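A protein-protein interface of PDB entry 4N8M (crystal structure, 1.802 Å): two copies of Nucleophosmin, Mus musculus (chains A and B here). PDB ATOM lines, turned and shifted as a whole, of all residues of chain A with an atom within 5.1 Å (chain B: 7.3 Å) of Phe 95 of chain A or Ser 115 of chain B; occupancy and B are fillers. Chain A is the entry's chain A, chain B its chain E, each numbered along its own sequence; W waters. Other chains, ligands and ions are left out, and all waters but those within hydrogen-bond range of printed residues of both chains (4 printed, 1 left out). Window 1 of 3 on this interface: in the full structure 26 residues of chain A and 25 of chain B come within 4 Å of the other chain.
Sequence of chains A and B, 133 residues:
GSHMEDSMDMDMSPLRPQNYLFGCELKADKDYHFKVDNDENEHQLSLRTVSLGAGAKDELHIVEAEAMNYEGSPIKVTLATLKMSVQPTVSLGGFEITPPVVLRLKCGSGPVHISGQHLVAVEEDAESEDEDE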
ATOM      1  N   LEU A  45      -4.425 -22.897  30.880  1.00  0.00           N
ATOM      2  CA  LEU A  45      -3.358 -21.904  30.780  1.00  0.00           C
ATOM      3  C   LEU A  45      -3.383 -21.377  29.337  1.00  0.00           C
ATOM      4  O   LEU A  45      -3.247 -22.153  28.392  1.00  0.00           O
ATOM      5  CB  LEU A  45      -2.021 -22.570  31.111  1.00  0.00           C
ATOM      6  CG  LEU A  45      -0.777 -21.682  31.085  1.00  0.00           C
ATOM      7  CD1 LEU A  45      -0.863 -20.634  32.186  1.00  0.00           C
ATOM      8  CD2 LEU A  45       0.490 -22.522  31.239  1.00  0.00           C
ATOM      9  N   SER A  46      -3.576 -20.072  29.152  1.00  0.00           N
ATOM     10  CA  SER A  46      -3.592 -19.503  27.805  1.00  0.00           C
ATOM     11  C   SER A  46      -2.366 -18.609  27.590  1.00  0.00           C
ATOM     12  O   SER A  46      -2.334 -17.469  28.073  1.00  0.00           O
ATOM     13  CB  SER A  46      -4.850 -18.692  27.574  1.00  0.00           C
ATOM     14  OG  SER A  46      -4.882 -18.222  26.241  1.00  0.00           O
ATOM     15  N   LEU A  47      -1.369 -19.115  26.868  1.00  0.00           N
ATOM     16  CA  LEU A  47      -0.089 -18.401  26.743  1.00  0.00           C
ATOM     17  C   LEU A  47      -0.188 -17.289  25.719  1.00  0.00           C
ATOM     18  O   LEU A  47      -0.745 -17.482  24.642  1.00  0.00           O
ATOM     19  CB  LEU A  47       1.044 -19.365  26.357  1.00  0.00           C
ATOM     20  CG  LEU A  47       1.228 -20.532  27.334  1.00  0.00           C
ATOM     21  CD1 LEU A  47       2.339 -21.452  26.849  1.00  0.00           C
ATOM     22  CD2 LEU A  47       1.515 -20.013  28.734  1.00  0.00           C
ATOM     23  N   VAL A  77       6.834 -30.168  23.272  1.00  0.00           N
ATOM     24  CA  VAL A  77       6.705 -29.384  22.050  1.00  0.00           C
ATOM     25  C   VAL A  77       7.482 -28.082  22.192  1.00  0.00           C
ATOM     26  O   VAL A  77       7.643 -27.565  23.292  1.00  0.00           O
ATOM     27  CB  VAL A  77       5.223 -29.075  21.712  1.00  0.00           C
ATOM     28  CG1 VAL A  77       4.362 -30.311  21.941  1.00  0.00           C
ATOM     29  CG2 VAL A  77       4.704 -27.905  22.541  1.00  0.00           C
ATOM     30  N   THR A  78       7.970 -27.559  21.075  1.00  0.00           N
ATOM     31  CA  THR A  78       8.637 -26.263  21.071  1.00  0.00           C
ATOM     32  C   THR A  78       7.627 -25.130  20.901  1.00  0.00           C
ATOM     33  O   THR A  78       6.880 -25.121  19.935  1.00  0.00           O
ATOM     34  CB  THR A  78       9.691 -26.220  19.940  1.00  0.00           C
ATOM     35  OG1 THR A  78      10.698 -27.195  20.216  1.00  0.00           O
ATOM     36  CG2 THR A  78      10.353 -24.848  19.845  1.00  0.00           C
ATOM     37  N   LEU A  79       7.610 -24.174  21.833  1.00  0.00           N
ATOM     38  CA  LEU A  79       6.685 -23.046  21.766  1.00  0.00           C
ATOM     39  C   LEU A  79       7.264 -21.924  20.907  1.00  0.00           C
ATOM     40  O   LEU A  79       6.547 -21.271  20.147  1.00  0.00           O
ATOM     41  CB  LEU A  79       6.396 -22.487  23.161  1.00  0.00           C
ATOM     42  CG  LEU A  79       5.671 -23.381  24.170  1.00  0.00           C
ATOM     43  CD1 LEU A  79       5.338 -22.584  25.425  1.00  0.00           C
ATOM     44  CD2 LEU A  79       4.410 -23.942  23.559  1.00  0.00           C
ATOM     45  N   LEU A  92       2.010 -15.515  21.030  1.00  0.00           N
ATOM     46  CA  LEU A  92       1.395 -16.813  20.735  1.00  0.00           C
ATOM     47  C   LEU A  92      -0.102 -16.717  20.499  1.00  0.00           C
ATOM     48  O   LEU A  92      -0.712 -17.646  19.969  1.00  0.00           O
ATOM     49  CB  LEU A  92       1.670 -17.797  21.872  1.00  0.00           C
ATOM     50  CG  LEU A  92       3.138 -18.105  22.159  1.00  0.00           C
ATOM     51  CD1 LEU A  92       3.305 -18.894  23.454  1.00  0.00           C
ATOM     52  CD2 LEU A  92       3.752 -18.853  20.968  1.00  0.00           C
ATOM     53  N   GLY A  93      -0.702 -15.600  20.892  1.00  0.00           N
ATOM     54  CA  GLY A  93      -2.090 -15.359  20.543  1.00  0.00           C
ATOM     55  C   GLY A  93      -3.101 -16.177  21.335  1.00  0.00           C
ATOM     56  O   GLY A  93      -4.217 -16.408  20.886  1.00  0.00           O
ATOM     57  N   GLY A  94      -2.735 -16.601  22.535  1.00  0.00           N
ATOM     58  CA  GLY A  94      -3.695 -17.351  23.332  1.00  0.00           C
ATOM     59  C   GLY A  94      -3.639 -18.835  23.035  1.00  0.00           C
ATOM     60  O   GLY A  94      -4.637 -19.441  22.635  1.00  0.00           O
ATOM     61  N   PHE A  95      -2.465 -19.421  23.248  1.00  0.00           N
ATOM     62  CA  PHE A  95      -2.244 -20.849  23.033  1.00  0.00           C
ATOM     63  C   PHE A  95      -2.688 -21.565  24.315  1.00  0.00           C
ATOM     64  O   PHE A  95      -1.993 -21.517  25.326  1.00  0.00           O
ATOM     65  CB  PHE A  95      -0.749 -21.035  22.795  1.00  0.00           C
ATOM     66  CG  PHE A  95      -0.331 -22.420  22.385  1.00  0.00           C
ATOM     67  CD1 PHE A  95       0.874 -22.607  21.713  1.00  0.00           C
ATOM     68  CD2 PHE A  95      -1.093 -23.536  22.708  1.00  0.00           C
ATOM     69  CE1 PHE A  95       1.292 -23.883  21.349  1.00  0.00           C
ATOM     70  CE2 PHE A  95      -0.674 -24.812  22.354  1.00  0.00           C
ATOM     71  CZ  PHE A  95       0.514 -24.985  21.667  1.00  0.00           C
ATOM     72  N   GLU A  96      -3.850 -22.204  24.279  1.00  0.00           N
ATOM     73  CA  GLU A  96      -4.399 -22.834  25.482  1.00  0.00           C
ATOM     74  C   GLU A  96      -3.856 -24.240  25.704  1.00  0.00           C
ATOM     75  O   GLU A  96      -3.742 -25.022  24.761  1.00  0.00           O
ATOM     76  CB  GLU A  96      -5.922 -22.895  25.404  1.00  0.00           C
ATOM     77  CG  GLU A  96      -6.564 -21.518  25.558  1.00  0.00           C
ATOM     78  CD  GLU A  96      -8.066 -21.556  25.378  1.00  0.00           C
ATOM     79  OE1 GLU A  96      -8.551 -21.026  24.355  1.00  0.00           O
ATOM     80  OE2 GLU A  96      -8.756 -22.114  26.260  1.00  0.00           O
ATOM     81  N   ILE A  97      -3.527 -24.542  26.958  1.00  0.00           N
ATOM     82  CA  ILE A  97      -3.047 -25.858  27.369  1.00  0.00           C
ATOM     83  C   ILE A  97      -3.715 -26.261  28.692  1.00  0.00           C
ATOM     84  O   ILE A  97      -3.882 -25.438  29.601  1.00  0.00           O
ATOM     85  CB  ILE A  97      -1.501 -25.893  27.516  1.00  0.00           C
ATOM     86  CG1 ILE A  97      -0.806 -25.282  26.289  1.00  0.00           C
ATOM     87  CG2 ILE A  97      -1.016 -27.330  27.723  1.00  0.00           C
ATOM     88  CD1 ILE A  97       0.678 -25.094  26.469  1.00  0.00           C
ATOM     89  N   ASN B  19      -9.115 -30.431  24.750  1.00  0.00           N
ATOM     90  CA  ASN B  19      -7.960 -29.744  24.210  1.00  0.00           C
ATOM     91  C   ASN B  19      -6.674 -30.446  24.625  1.00  0.00           C
ATOM     92  O   ASN B  19      -6.372 -30.535  25.814  1.00  0.00           O
ATOM     93  CB  ASN B  19      -7.957 -28.303  24.733  1.00  0.00           C
ATOM     94  CG  ASN B  19      -6.731 -27.547  24.321  1.00  0.00           C
ATOM     95  OD1 ASN B  19      -6.133 -27.840  23.292  1.00  0.00           O
ATOM     96  ND2 ASN B  19      -6.320 -26.574  25.146  1.00  0.00           N
ATOM     97  N   TYR B  20      -5.923 -30.944  23.647  1.00  0.00           N
ATOM     98  CA  TYR B  20      -4.693 -31.675  23.901  1.00  0.00           C
ATOM     99  C   TYR B  20      -3.534 -31.015  23.191  1.00  0.00           C
ATOM    100  O   TYR B  20      -3.704 -30.369  22.159  1.00  0.00           O
ATOM    101  CB  TYR B  20      -4.817 -33.135  23.419  1.00  0.00           C
ATOM    102  CG  TYR B  20      -5.989 -33.843  24.056  1.00  0.00           C
ATOM    103  CD1 TYR B  20      -7.236 -33.838  23.451  1.00  0.00           C
ATOM    104  CD2 TYR B  20      -5.852 -34.480  25.287  1.00  0.00           C
ATOM    105  CE1 TYR B  20      -8.319 -34.473  24.050  1.00  0.00           C
ATOM    106  CE2 TYR B  20      -6.919 -35.109  25.888  1.00  0.00           C
ATOM    107  CZ  TYR B  20      -8.149 -35.103  25.269  1.00  0.00           C
ATOM    108  OH  TYR B  20      -9.210 -35.729  25.878  1.00  0.00           O
ATOM    109  N   LEU B  21      -2.343 -31.193  23.737  1.00  0.00           N
ATOM    110  CA  LEU B  21      -1.170 -30.538  23.167  1.00  0.00           C
ATOM    111  C   LEU B  21      -0.678 -31.353  21.974  1.00  0.00           C
ATOM    112  O   LEU B  21      -0.716 -32.593  21.995  1.00  0.00           O
ATOM    113  CB  LEU B  21      -0.079 -30.434  24.216  1.00  0.00           C
ATOM    114  CG  LEU B  21       1.176 -29.666  23.809  1.00  0.00           C
ATOM    115  CD1 LEU B  21       0.838 -28.184  23.634  1.00  0.00           C
ATOM    116  CD2 LEU B  21       2.267 -29.864  24.831  1.00  0.00           C
ATOM    117  N   PHE B  22      -0.219 -30.659  20.941  1.00  0.00           N
ATOM    118  CA  PHE B  22       0.306 -31.307  19.746  1.00  0.00           C
ATOM    119  C   PHE B  22       1.677 -30.735  19.373  1.00  0.00           C
ATOM    120  O   PHE B  22       1.924 -29.548  19.533  1.00  0.00           O
ATOM    121  CB  PHE B  22      -0.638 -31.102  18.562  1.00  0.00           C
ATOM    122  CG  PHE B  22      -0.020 -31.494  17.246  1.00  0.00           C
ATOM    123  CD1 PHE B  22      -0.016 -32.817  16.839  1.00  0.00           C
ATOM    124  CD2 PHE B  22       0.603 -30.541  16.443  1.00  0.00           C
ATOM    125  CE1 PHE B  22       0.575 -33.183  15.639  1.00  0.00           C
ATOM    126  CE2 PHE B  22       1.195 -30.897  15.242  1.00  0.00           C
ATOM    127  CZ  PHE B  22       1.185 -32.218  14.840  1.00  0.00           C
ATOM    128  N   GLY B  23       2.569 -31.572  18.861  1.00  0.00           N
ATOM    129  CA  GLY B  23       3.826 -31.051  18.342  1.00  0.00           C
ATOM    130  C   GLY B  23       4.481 -32.067  17.429  1.00  0.00           C
ATOM    131  O   GLY B  23       4.253 -33.271  17.568  1.00  0.00           O
ATOM    132  N   CYS B  24       5.278 -31.590  16.483  1.00  0.00           N
ATOM    133  CA  CYS B  24       6.127 -32.505  15.711  1.00  0.00           C
ATOM    134  C   CYS B  24       7.419 -31.823  15.293  1.00  0.00           C
ATOM    135  O   CYS B  24       7.553 -30.603  15.373  1.00  0.00           O
ATOM    136  CB  CYS B  24       5.384 -33.034  14.484  1.00  0.00           C
ATOM    137  SG  CYS B  24       4.913 -31.777  13.277  1.00  0.00           S
ATOM    138  N   LEU B  45      -6.853 -30.122  14.000  1.00  0.00           N
ATOM    139  CA  LEU B  45      -5.498 -29.744  14.378  1.00  0.00           C
ATOM    140  C   LEU B  45      -5.430 -28.237  14.267  1.00  0.00           C
ATOM    141  O   LEU B  45      -5.707 -27.690  13.203  1.00  0.00           O
ATOM    142  CB  LEU B  45      -4.493 -30.397  13.426  1.00  0.00           C
ATOM    143  CG  LEU B  45      -3.021 -30.026  13.587  1.00  0.00           C
ATOM    144  CD1 LEU B  45      -2.550 -30.275  15.010  1.00  0.00           C
ATOM    145  CD2 LEU B  45      -2.152 -30.797  12.579  1.00  0.00           C
ATOM    146  N   SER B  46      -5.095 -27.558  15.361  1.00  0.00           N
ATOM    147  CA  SER B  46      -4.964 -26.102  15.347  1.00  0.00           C
ATOM    148  C   SER B  46      -3.498 -25.720  15.540  1.00  0.00           C
ATOM    149  O   SER B  46      -2.952 -25.849  16.631  1.00  0.00           O
ATOM    150  CB  SER B  46      -5.828 -25.469  16.445  1.00  0.00           C
ATOM    151  OG  SER B  46      -5.700 -24.063  16.415  1.00  0.00           O
ATOM    152  N   LEU B  47      -2.860 -25.263  14.467  1.00  0.00           N
ATOM    153  CA  LEU B  47      -1.433 -24.976  14.494  1.00  0.00           C
ATOM    154  C   LEU B  47      -1.156 -23.637  15.157  1.00  0.00           C
ATOM    155  O   LEU B  47      -1.836 -22.639  14.881  1.00  0.00           O
ATOM    156  CB  LEU B  47      -0.866 -24.977  13.068  1.00  0.00           C
ATOM    157  CG  LEU B  47      -1.027 -26.304  12.324  1.00  0.00           C
ATOM    158  CD1 LEU B  47      -0.487 -26.189  10.903  1.00  0.00           C
ATOM    159  CD2 LEU B  47      -0.319 -27.430  13.073  1.00  0.00           C
ATOM    160  N   ARG B  48      -0.149 -23.606  16.024  1.00  0.00           N
ATOM    161  CA  ARG B  48       0.185 -22.373  16.733  1.00  0.00           C
ATOM    162  C   ARG B  48       1.507 -21.742  16.291  1.00  0.00           C
ATOM    163  O   ARG B  48       1.520 -20.605  15.858  1.00  0.00           O
ATOM    164  CB  ARG B  48       0.227 -22.630  18.237  1.00  0.00           C
ATOM    165  CG  ARG B  48      -1.131 -22.797  18.825  1.00  0.00           C
ATOM    166  CD  ARG B  48      -1.704 -21.389  19.037  1.00  0.00           C
ATOM    167  NE  ARG B  48      -3.129 -21.462  19.228  1.00  0.00           N
ATOM    168  CZ  ARG B  48      -3.908 -20.406  19.384  1.00  0.00           C
ATOM    169  NH1 ARG B  48      -3.385 -19.180  19.384  1.00  0.00           N
ATOM    170  NH2 ARG B  48      -5.200 -20.590  19.540  1.00  0.00           N
ATOM    171  N   THR B  49       2.620 -22.452  16.439  1.00  0.00           N
ATOM    172  CA  THR B  49       3.901 -21.878  16.012  1.00  0.00           C
ATOM    173  C   THR B  49       4.705 -22.832  15.151  1.00  0.00           C
ATOM    174  O   THR B  49       4.553 -24.057  15.216  1.00  0.00           O
ATOM    175  CB  THR B  49       4.814 -21.439  17.185  1.00  0.00           C
ATOM    176  OG1 THR B  49       5.156 -22.576  17.981  1.00  0.00           O
ATOM    177  CG2 THR B  49       4.112 -20.414  18.046  1.00  0.00           C
ATOM    178  N   VAL B  50       5.561 -22.235  14.341  1.00  0.00           N
ATOM    179  CA  VAL B  50       6.516 -22.959  13.529  1.00  0.00           C
ATOM    180  C   VAL B  50       7.833 -22.296  13.909  1.00  0.00           C
ATOM    181  O   VAL B  50       7.956 -21.078  13.812  1.00  0.00           O
ATOM    182  CB  VAL B  50       6.187 -22.740  12.038  1.00  0.00           C
ATOM    183  CG1 VAL B  50       7.092 -23.582  11.166  1.00  0.00           C
ATOM    184  CG2 VAL B  50       4.725 -23.109  11.773  1.00  0.00           C
ATOM    185  N   SER B  51       8.807 -23.069  14.377  1.00  0.00           N
ATOM    186  CA  SER B  51      10.055 -22.507  14.899  1.00  0.00           C
ATOM    187  C   SER B  51      11.259 -23.324  14.425  1.00  0.00           C
ATOM    188  O   SER B  51      11.178 -24.549  14.355  1.00  0.00           O
ATOM    189  CB  SER B  51      10.042 -22.513  16.436  1.00  0.00           C
ATOM    190  OG  SER B  51       8.829 -21.993  16.972  1.00  0.00           O
ATOM    191  N   VAL B  90       7.442 -18.236  13.524  1.00  0.00           N
ATOM    192  CA  VAL B  90       6.239 -17.652  12.991  1.00  0.00           C
ATOM    193  C   VAL B  90       5.085 -18.170  13.852  1.00  0.00           C
ATOM    194  O   VAL B  90       4.982 -19.370  14.110  1.00  0.00           O
ATOM    195  CB  VAL B  90       6.049 -18.101  11.517  1.00  0.00           C
ATOM    196  CG1 VAL B  90       4.623 -17.859  11.049  1.00  0.00           C
ATOM    197  CG2 VAL B  90       7.048 -17.375  10.622  1.00  0.00           C
ATOM    198  N   LEU B  92       1.111 -18.726  14.052  1.00  0.00           N
ATOM    199  CA  LEU B  92      -0.023 -18.823  13.121  1.00  0.00           C
ATOM    200  C   LEU B  92      -1.366 -18.433  13.730  1.00  0.00           C
ATOM    201  O   LEU B  92      -2.360 -18.253  13.012  1.00  0.00           O
ATOM    202  CB  LEU B  92      -0.122 -20.237  12.568  1.00  0.00           C
ATOM    203  CG  LEU B  92       1.163 -20.752  11.937  1.00  0.00           C
ATOM    204  CD1 LEU B  92       1.035 -22.239  11.596  1.00  0.00           C
ATOM    205  CD2 LEU B  92       1.444 -19.923  10.691  1.00  0.00           C
ATOM    206  N   HIS B 113      10.297 -27.113  14.169  1.00  0.00           N
ATOM    207  CA  HIS B 113       9.302 -27.620  15.109  1.00  0.00           C
ATOM    208  C   HIS B 113       7.952 -27.004  14.824  1.00  0.00           C
ATOM    209  O   HIS B 113       7.866 -25.850  14.404  1.00  0.00           O
ATOM    210  CB  HIS B 113       9.723 -27.312  16.546  1.00  0.00           C
ATOM    211  CG  HIS B 113      10.932 -28.074  16.987  1.00  0.00           C
ATOM    212  ND1 HIS B 113      12.185 -27.505  17.062  1.00  0.00           N
ATOM    213  CD2 HIS B 113      11.086 -29.371  17.346  1.00  0.00           C
ATOM    214  CE1 HIS B 113      13.058 -28.415  17.458  1.00  0.00           C
ATOM    215  NE2 HIS B 113      12.417 -29.556  17.635  1.00  0.00           N
ATOM    216  N   ILE B 114       6.901 -27.786  15.007  1.00  0.00           N
ATOM    217  CA  ILE B 114       5.554 -27.263  14.926  1.00  0.00           C
ATOM    218  C   ILE B 114       4.871 -27.531  16.260  1.00  0.00           C
ATOM    219  O   ILE B 114       5.021 -28.613  16.839  1.00  0.00           O
ATOM    220  CB  ILE B 114       4.772 -27.940  13.796  1.00  0.00           C
ATOM    221  CG1 ILE B 114       5.494 -27.707  12.465  1.00  0.00           C
ATOM    222  CG2 ILE B 114       3.331 -27.402  13.735  1.00  0.00           C
ATOM    223  CD1 ILE B 114       4.586 -27.688  11.264  1.00  0.00           C
ATOM    224  N   SER B 115       4.139 -26.548  16.768  1.00  0.00           N
ATOM    225  CA  SER B 115       3.338 -26.778  17.964  1.00  0.00           C
ATOM    226  C   SER B 115       1.892 -26.379  17.706  1.00  0.00           C
ATOM    227  O   SER B 115       1.602 -25.567  16.823  1.00  0.00           O
ATOM    228  CB  SER B 115       3.887 -25.962  19.133  1.00  0.00           C
ATOM    229  OG  SER B 115       3.609 -24.583  18.938  1.00  0.00           O
ATOM    230  N   GLY B 116       0.974 -26.937  18.482  1.00  0.00           N
ATOM    231  CA  GLY B 116      -0.408 -26.525  18.364  1.00  0.00           C
ATOM    232  C   GLY B 116      -1.275 -27.336  19.297  1.00  0.00           C
ATOM    233  O   GLY B 116      -0.788 -27.912  20.263  1.00  0.00           O
ATOM    234  N   GLN B 117      -2.559 -27.384  18.984  1.00  0.00           N
ATOM    235  CA  GLN B 117      -3.531 -28.064  19.824  1.00  0.00           C
ATOM    236  C   GLN B 117      -4.235 -29.137  19.010  1.00  0.00           C
ATOM    237  O   GLN B 117      -4.573 -28.927  17.847  1.00  0.00           O
ATOM    238  CB  GLN B 117      -4.548 -27.067  20.365  1.00  0.00           C
ATOM    239  CG  GLN B 117      -3.912 -25.882  21.093  1.00  0.00           C
ATOM    240  CD  GLN B 117      -4.914 -24.797  21.480  1.00  0.00           C
ATOM    241  OE1 GLN B 117      -4.622 -23.608  21.381  1.00  0.00           O
ATOM    242  NE2 GLN B 117      -6.080 -25.203  21.954  1.00  0.00           N
ATOM    243  N   HIS B 118      -4.442 -30.288  19.623  1.00  0.00           N
ATOM    244  CA  HIS B 118      -5.350 -31.285  19.058  1.00  0.00           C
ATOM    245  C   HIS B 118      -6.700 -31.111  19.741  1.00  0.00           C
ATOM    246  O   HIS B 118      -6.843 -31.399  20.936  1.00  0.00           O
ATOM    247  CB  HIS B 118      -4.789 -32.695  19.264  1.00  0.00           C
ATOM    248  CG  HIS B 118      -5.632 -33.781  18.664  1.00  0.00           C
ATOM    249  ND1 HIS B 118      -5.255 -35.106  18.666  1.00  0.00           N
ATOM    250  CD2 HIS B 118      -6.837 -33.736  18.045  1.00  0.00           C
ATOM    251  CE1 HIS B 118      -6.190 -35.833  18.081  1.00  0.00           C
ATOM    252  NE2 HIS B 118      -7.157 -35.025  17.686  1.00  0.00           N
HETATM  253  O   HOH W   1      -6.031 -21.633  22.220  1.00  0.00           O
HETATM  254  O   HOH W   2       7.273 -24.446  17.114  1.00  0.00           O
HETATM  255  O   HOH W   3       7.269 -29.012  18.597  1.00  0.00           O
HETATM  256  O   HOH W   4       0.060 -19.070  17.690  1.00  0.00           O
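Of the printed residues of chain B, Gly 93 of chain A touches Arg 48 (3.3 Å).
Of chain B, only Arg 48 (3.3 Å) comes within 4 Å of Gly 94 of chain A.
Phe 95 of chain A touches just these residues of chain B: Leu 21 (3.8 Å), Arg 48 (3.5 Å), Ser 115 (3.4 Å), Gly 116 (3.5 Å) and Gln 117 (3.6 Å).
Printed residues of chain A within 4 Å of Asn 19 of chain B: Glu 96 and Ile 97.
Printed residues of chain A within 4 Å of Ser 115 of chain B: Thr 78 (3.2 Å) and Phe 95 (3.4 Å).
Of the printed residues of chain A, Gly 116 of chain B touches Phe 95 (3.5 Å).
The nearest residue of chain B that does not touch Phe 95 of chain A is Phe 22 of chain B (5.2 Å).
The nearest printed residue of chain A that does not touch Ser 115 of chain B is Val 77 of chain A (4.01 Å).
Water W1 lies within hydrogen-bond range of the side-chain amide oxygen of Gln 117 of chain B (2.6 Å), the backbone carbonyl oxygen of Gly 94 of chain A (2.6 Å), the guanidinium group of Arg 48 of chain B (3.0 Å) and the backbone NH of Glu 96 of chain A (3.1 Å).
Water W4 bridges O of Leu 92 of chain A and O of Arg 48 of chain B.
Water W3 lies within hydrogen-bond range of O of Ile 114 of chain B (2.9 Å) and N of Thr 78 of chain A (3.0 Å).
Water W2 lies within hydrogen-bond range of the side-chain hydroxyl of Ser 51 of chain B (2.9 Å), the backbone carbonyl oxygen of Thr 78 of chain A (2.9 Å), the side-chain hydroxyl of Thr 49 of chain B (3.0 Å) and the backbone carbonyl oxygen of His 113 of chain B (3.1 Å).
The backbone carbonyl oxygen of Leu 45 of chain A lies within hydrogen-bond range of the backbone NH of Ile 97 of chain A (2.8 Å).
The backbone carbonyl oxygen of Leu 47 of chain A sits at hydrogen-bond distance from the backbone NH of Gly 94 of chain A (3.0 Å).
The backbone carbonyl oxygen (O) of Gly 116 of chain B is in hydrogen-bond range of the backbone NH (N) of Phe 22 of chain B (2.9 Å).
The backbone NH of Arg 48 of chain B sits at hydrogen-bond distance from the backbone carbonyl oxygen of Ser 115 of chain B.
The side-chain hydroxyl (OG) of Ser 115 of chain B sits at hydrogen-bond distance from the side-chain hydroxyl (OG1) of Thr 49 of chain B (2.7 Å).
The backbone NH (N) of His 113 of chain B lies within hydrogen-bond range of the backbone carbonyl oxygen (O) of Ser 51 of chain B (2.7 Å).
The backbone carbonyl oxygen of Thr 78 of chain A lies close to the side-chain hydroxyl of Ser 115 of chain B, at 3.5 Å.
OG1 of Thr 49 of chain B sits at hydrogen-bond distance from O of Leu 79 of chain A, at 2.9 Å.
The backbone carbonyl oxygen (O) of Leu 92 of chain A sits at hydrogen-bond distance from the guanidinium group (NH1) of Arg 48 of chain B, at 3.1 Å.
The backbone carbonyl oxygen of Gly 93 of chain A is in hydrogen-bond range of the guanidinium group of Arg 48 of chain B, at 3.3 Å.
The backbone carbonyl oxygen (O) of Gly 94 of chain A is in hydrogen-bond range of the guanidinium group (NH2) of Arg 48 of chain B, at 3.3 Å.
The backbone carbonyl oxygen of Glu 96 of chain A sits at hydrogen-bond distance from the side-chain amide nitrogen of Asn 19 of chain B (3.0 Å).
OE1 of Gln 117 of chain B sits at hydrogen-bond distance from N of Glu 96 of chain A, at 3.3 Å.
Positions printed for both chains: 45, 46, 47 and 92.
Among the printed residues, merely in contact across the chains: Leu 92 of chain A with Thr 49 of chain B (3.3 Å), Thr 78 of chain A with His 113 of chain B (3.4 Å), Phe 95 of chain A with Ser 115 of chain B (3.4 Å), Phe 95 of chain A with Gly 116 of chain B (3.5 Å), Val 77 of chain A with Phe 22 of chain B (3.5 Å), Phe 95 of chain A with Arg 48 of chain B (3.5 Å), Val 77 of chain A with Leu 21 of chain B (3.6 Å), Phe 95 of chain A with Gln 117 of chain B (3.6 Å), Thr 78 of chain A with Thr 49 of chain B (3.6 Å), Val 77 of chain A with Gly 23 of chain B (3.7 Å), Phe 95 of chain A with Leu 21 of chain B (3.8 Å), Ile 97 of chain A with Asn 19 of chain B (3.9 Å) and Leu 79 of chain A with Ser 51 of chain B (3.98 Å).
Of the 21 printed residues of chain B, 11 touch a printed residue of chain A.
Printed residues of chain A that touch a printed residue of chain B: Val 77, Thr 78, Leu 79, Leu 92, Gly 93, Gly 94, Phe 95, Glu 96 and Ile 97.
Hydrophobic or aromatic side chains of chain A within 4 Å of the printed part of chain B: Val 77, Leu 92 and Phe 95.
Along chain A the printed residues that touch a printed residue of chain B span positions 77 to 97.
Among the printed residues, no Asp or Glu carboxylate lies within 4 Å of a Lys or Arg side-chain nitrogen of the other chain.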
